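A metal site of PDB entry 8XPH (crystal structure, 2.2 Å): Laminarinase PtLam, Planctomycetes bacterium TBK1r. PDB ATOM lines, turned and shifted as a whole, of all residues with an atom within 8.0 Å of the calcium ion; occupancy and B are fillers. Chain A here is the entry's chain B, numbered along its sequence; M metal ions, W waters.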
ATOM      1  N   GLN A  12      -8.301  13.913   0.015  1.00  0.00           N
ATOM      2  CA  GLN A  12      -7.793  13.999   1.369  1.00  0.00           C
ATOM      3  C   GLN A  12      -7.124  15.364   1.513  1.00  0.00           C
ATOM      4  O   GLN A  12      -6.139  15.653   0.831  1.00  0.00           O
ATOM      5  CB  GLN A  12      -6.816  12.857   1.653  1.00  0.00           C
ATOM      6  CG  GLN A  12      -7.480  11.501   1.832  1.00  0.00           C
ATOM      7  CD  GLN A  12      -8.230  11.359   3.139  1.00  0.00           C
ATOM      8  OE1 GLN A  12      -9.455  11.258   3.172  1.00  0.00           O
ATOM      9  NE2 GLN A  12      -7.481  11.364   4.234  1.00  0.00           N
ATOM     10  N   GLU A  13      -7.689  16.217   2.383  1.00  0.00           N
ATOM     11  CA  GLU A  13      -7.221  17.578   2.558  1.00  0.00           C
ATOM     12  C   GLU A  13      -6.199  17.665   3.685  1.00  0.00           C
ATOM     13  O   GLU A  13      -5.521  18.683   3.814  1.00  0.00           O
ATOM     14  CB  GLU A  13      -8.415  18.495   2.810  1.00  0.00           C
ATOM     15  CG  GLU A  13      -9.375  18.597   1.623  1.00  0.00           C
ATOM     16  CD  GLU A  13      -8.780  19.188   0.363  1.00  0.00           C
ATOM     17  OE1 GLU A  13      -7.985  20.154   0.461  1.00  0.00           O
ATOM     18  OE2 GLU A  13      -9.144  18.722  -0.731  1.00  0.00           O
ATOM     19  N   PHE A  14      -6.125  16.614   4.512  1.00  0.00           N
ATOM     20  CA  PHE A  14      -5.131  16.495   5.580  1.00  0.00           C
ATOM     21  C   PHE A  14      -5.268  17.680   6.545  1.00  0.00           C
ATOM     22  O   PHE A  14      -4.263  18.211   6.984  1.00  0.00           O
ATOM     23  CB  PHE A  14      -3.707  16.420   5.017  1.00  0.00           C
ATOM     24  CG  PHE A  14      -3.443  15.284   4.045  1.00  0.00           C
ATOM     25  CD1 PHE A  14      -3.513  13.953   4.467  1.00  0.00           C
ATOM     26  CD2 PHE A  14      -3.097  15.535   2.721  1.00  0.00           C
ATOM     27  CE1 PHE A  14      -3.273  12.907   3.581  1.00  0.00           C
ATOM     28  CE2 PHE A  14      -2.857  14.488   1.836  1.00  0.00           C
ATOM     29  CZ  PHE A  14      -2.952  13.173   2.266  1.00  0.00           C
ATOM     30  N   ASP A  15      -6.508  18.056   6.872  1.00  0.00           N
ATOM     31  CA  ASP A  15      -6.770  19.236   7.699  1.00  0.00           C
ATOM     32  C   ASP A  15      -7.022  18.847   9.153  1.00  0.00           C
ATOM     33  O   ASP A  15      -7.011  19.721  10.012  1.00  0.00           O
ATOM     34  CB  ASP A  15      -7.904  20.075   7.120  1.00  0.00           C
ATOM     35  CG  ASP A  15      -7.559  20.870   5.868  1.00  0.00           C
ATOM     36  OD1 ASP A  15      -6.355  21.080   5.611  1.00  0.00           O
ATOM     37  OD2 ASP A  15      -8.498  21.256   5.149  1.00  0.00           O
ATOM     38  N   GLY A  16      -7.247  17.555   9.413  1.00  0.00           N
ATOM     39  CA  GLY A  16      -7.563  17.087  10.758  1.00  0.00           C
ATOM     40  C   GLY A  16      -6.321  17.009  11.644  1.00  0.00           C
ATOM     41  O   GLY A  16      -5.337  17.707  11.423  1.00  0.00           O
ATOM     42  N   ARG A  51      -0.315  18.183  10.373  1.00  0.00           N
ATOM     43  CA  ARG A  51      -0.122  19.446  11.079  1.00  0.00           C
ATOM     44  C   ARG A  51      -0.350  20.618  10.118  1.00  0.00           C
ATOM     45  O   ARG A  51       0.170  20.618   9.011  1.00  0.00           O
ATOM     46  CB  ARG A  51       1.280  19.433  11.700  1.00  0.00           C
ATOM     47  CG  ARG A  51       1.545  20.532  12.703  1.00  0.00           C
ATOM     48  CD  ARG A  51       2.945  20.449  13.270  1.00  0.00           C
ATOM     49  NE  ARG A  51       3.054  19.494  14.380  1.00  0.00           N
ATOM     50  CZ  ARG A  51       2.600  19.684  15.614  1.00  0.00           C
ATOM     51  NH1 ARG A  51       2.040  20.826  15.966  1.00  0.00           N
ATOM     52  NH2 ARG A  51       2.736  18.725  16.523  1.00  0.00           N
ATOM     53  N   ASP A  52      -1.182  21.576  10.556  1.00  0.00           N
ATOM     54  CA  ASP A  52      -1.357  22.862   9.897  1.00  0.00           C
ATOM     55  C   ASP A  52      -1.873  22.707   8.469  1.00  0.00           C
ATOM     56  O   ASP A  52      -1.534  23.487   7.584  1.00  0.00           O
ATOM     57  CB  ASP A  52      -0.061  23.671   9.951  1.00  0.00           C
ATOM     58  CG  ASP A  52       0.452  23.975  11.348  1.00  0.00           C
ATOM     59  OD1 ASP A  52      -0.373  24.420  12.179  1.00  0.00           O
ATOM     60  OD2 ASP A  52       1.656  23.784  11.580  1.00  0.00           O
ATOM     61  N   GLY A  53      -2.755  21.714   8.274  1.00  0.00           N
ATOM     62  CA  GLY A  53      -3.377  21.490   6.986  1.00  0.00           C
ATOM     63  C   GLY A  53      -2.472  20.717   6.024  1.00  0.00           C
ATOM     64  O   GLY A  53      -2.661  20.806   4.809  1.00  0.00           O
ATOM     65  N   ASN A  54      -1.516  19.962   6.573  1.00  0.00           N
ATOM     66  CA  ASN A  54      -0.548  19.220   5.775  1.00  0.00           C
ATOM     67  C   ASN A  54      -0.404  17.797   6.308  1.00  0.00           C
ATOM     68  O   ASN A  54      -0.420  17.566   7.513  1.00  0.00           O
ATOM     69  CB  ASN A  54       0.825  19.883   5.781  1.00  0.00           C
ATOM     70  CG  ASN A  54       0.853  21.135   4.952  1.00  0.00           C
ATOM     71  OD1 ASN A  54       0.654  21.072   3.735  1.00  0.00           O
ATOM     72  ND2 ASN A  54       1.126  22.280   5.568  1.00  0.00           N
ATOM     73  N   LEU A  55      -0.249  16.839   5.369  1.00  0.00           N
ATOM     74  CA  LEU A  55       0.396  15.579   5.662  1.00  0.00           C
ATOM     75  C   LEU A  55       1.907  15.808   5.617  1.00  0.00           C
ATOM     76  O   LEU A  55       2.407  16.408   4.674  1.00  0.00           O
ATOM     77  CB  LEU A  55      -0.012  14.473   4.686  1.00  0.00           C
ATOM     78  CG  LEU A  55       0.881  13.226   4.674  1.00  0.00           C
ATOM     79  CD1 LEU A  55       0.657  12.358   5.909  1.00  0.00           C
ATOM     80  CD2 LEU A  55       0.679  12.426   3.409  1.00  0.00           C
ATOM     81  N   ARG A  90      -0.740  18.639  -4.148  1.00  0.00           N
ATOM     82  CA  ARG A  90       0.091  19.799  -3.875  1.00  0.00           C
ATOM     83  C   ARG A  90       1.150  19.383  -2.858  1.00  0.00           C
ATOM     84  O   ARG A  90       0.837  19.135  -1.699  1.00  0.00           O
ATOM     85  CB  ARG A  90      -0.797  20.950  -3.379  1.00  0.00           C
ATOM     86  CG  ARG A  90      -0.071  22.275  -3.246  1.00  0.00           C
ATOM     87  CD  ARG A  90      -1.005  23.426  -2.923  1.00  0.00           C
ATOM     88  NE  ARG A  90      -0.290  24.706  -2.919  1.00  0.00           N
ATOM     89  CZ  ARG A  90       0.157  25.355  -1.846  1.00  0.00           C
ATOM     90  NH1 ARG A  90       0.033  24.833  -0.635  1.00  0.00           N
ATOM     91  NH2 ARG A  90       0.743  26.531  -1.992  1.00  0.00           N
ATOM     92  N   VAL A 244       2.479  17.420   2.116  1.00  0.00           N
ATOM     93  CA  VAL A 244       1.372  17.213   1.181  1.00  0.00           C
ATOM     94  C   VAL A 244       0.172  18.004   1.684  1.00  0.00           C
ATOM     95  O   VAL A 244      -0.397  17.669   2.729  1.00  0.00           O
ATOM     96  CB  VAL A 244       1.011  15.727   1.009  1.00  0.00           C
ATOM     97  CG1 VAL A 244      -0.014  15.530  -0.102  1.00  0.00           C
ATOM     98  CG2 VAL A 244       2.234  14.848   0.773  1.00  0.00           C
ATOM     99  N   ASP A 245      -0.205  19.052   0.950  1.00  0.00           N
ATOM    100  CA  ASP A 245      -1.313  19.909   1.346  1.00  0.00           C
ATOM    101  C   ASP A 245      -2.626  19.184   1.088  1.00  0.00           C
ATOM    102  O   ASP A 245      -3.538  19.248   1.905  1.00  0.00           O
ATOM    103  CB  ASP A 245      -1.262  21.265   0.640  1.00  0.00           C
ATOM    104  CG  ASP A 245      -2.287  22.297   1.100  1.00  0.00           C
ATOM    105  OD1 ASP A 245      -2.906  22.087   2.161  1.00  0.00           O
ATOM    106  OD2 ASP A 245      -2.469  23.296   0.376  1.00  0.00           O
ATOM    107  N   TRP A 246      -2.723  18.507  -0.061  1.00  0.00           N
ATOM    108  CA  TRP A 246      -3.913  17.742  -0.388  1.00  0.00           C
ATOM    109  C   TRP A 246      -3.653  16.828  -1.566  1.00  0.00           C
ATOM    110  O   TRP A 246      -2.669  17.001  -2.289  1.00  0.00           O
ATOM    111  CB  TRP A 246      -5.100  18.688  -0.673  1.00  0.00           C
ATOM    112  CG  TRP A 246      -4.787  19.875  -1.558  1.00  0.00           C
ATOM    113  CD1 TRP A 246      -4.562  21.157  -1.152  1.00  0.00           C
ATOM    114  CD2 TRP A 246      -4.715  19.892  -2.995  1.00  0.00           C
ATOM    115  NE1 TRP A 246      -4.345  21.968  -2.236  1.00  0.00           N
ATOM    116  CE2 TRP A 246      -4.429  21.212  -3.378  1.00  0.00           C
ATOM    117  CE3 TRP A 246      -4.851  18.917  -3.992  1.00  0.00           C
ATOM    118  CZ2 TRP A 246      -4.285  21.595  -4.708  1.00  0.00           C
ATOM    119  CZ3 TRP A 246      -4.720  19.294  -5.313  1.00  0.00           C
ATOM    120  CH2 TRP A 246      -4.443  20.619  -5.661  1.00  0.00           C
ATOM    121  N   ILE A 247      -4.526  15.821  -1.712  1.00  0.00           N
ATOM    122  CA  ILE A 247      -4.628  15.014  -2.920  1.00  0.00           C
ATOM    123  C   ILE A 247      -6.090  15.019  -3.344  1.00  0.00           C
ATOM    124  O   ILE A 247      -6.972  14.742  -2.530  1.00  0.00           O
ATOM    125  CB  ILE A 247      -4.061  13.590  -2.697  1.00  0.00           C
ATOM    126  CG1 ILE A 247      -4.102  12.775  -4.001  1.00  0.00           C
ATOM    127  CG2 ILE A 247      -4.724  12.864  -1.528  1.00  0.00           C
ATOM    128  CD1 ILE A 247      -3.523  11.378  -3.899  1.00  0.00           C
ATOM    129  N   ARG A 248      -6.349  15.354  -4.607  1.00  0.00           N
ATOM    130  CA  ARG A 248      -7.709  15.527  -5.080  1.00  0.00           C
ATOM    131  C   ARG A 248      -7.924  14.766  -6.382  1.00  0.00           C
ATOM    132  O   ARG A 248      -7.066  14.811  -7.268  1.00  0.00           O
ATOM    133  CB  ARG A 248      -7.992  17.014  -5.312  1.00  0.00           C
ATOM    134  CG  ARG A 248      -8.080  17.833  -4.032  1.00  0.00           C
ATOM    135  CD  ARG A 248      -8.198  19.328  -4.336  1.00  0.00           C
ATOM    136  NE  ARG A 248      -8.150  20.109  -3.092  1.00  0.00           N
ATOM    137  CZ  ARG A 248      -7.950  21.413  -3.016  1.00  0.00           C
ATOM    138  NH1 ARG A 248      -7.769  22.139  -4.115  1.00  0.00           N
ATOM    139  NH2 ARG A 248      -7.919  22.007  -1.834  1.00  0.00           N
HETATM  140 CA    CA M   1      -4.699  20.818   3.772  1.00  0.00          CA
HETATM  141  O   HOH W   1      -5.476  21.451   1.958  1.00  0.00           O
HETATM  142  O   HOH W   2      -4.497  23.635   3.536  1.00  0.00           O
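OE2 of Glu 13 lies within salt-bridge range of NE of Arg 248 (2.9 Å). OD2 of Asp 245 sits close to NE1 of Trp 246, 3.5 Å away. The side-chain carboxylate of Asp 245 is in salt-bridge range of the guanidinium group of Arg 90, at 3.1 Å.
Of the 16 residues printed, 4 come within 4 Å of the calcium ion. Along chain A the residues within 4 Å of the calcium ion span positions 13 to 245. The nearest printed residue that does not touch the calcium ion is Phe 14 (4.2 Å).
Water W1 binds the calcium ion, 2.1 Å away. O of Gly 53 is bound to the calcium ion (2.3 Å). The calcium ion is bound by the backbone carbonyl oxygen (O) of Glu 13, at 2.3 Å. The calcium ion is bound by the side-chain carboxylate (OD1) of Asp 15 (2.5 Å). The calcium ion is bound by the backbone carbonyl oxygen (O) of Asp 245 (2.7 Å). The side-chain carboxylate (OD1) of Asp 245 binds the calcium ion (2.7 Å). The calcium ion is bound by water W2, at 2.8 Å.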
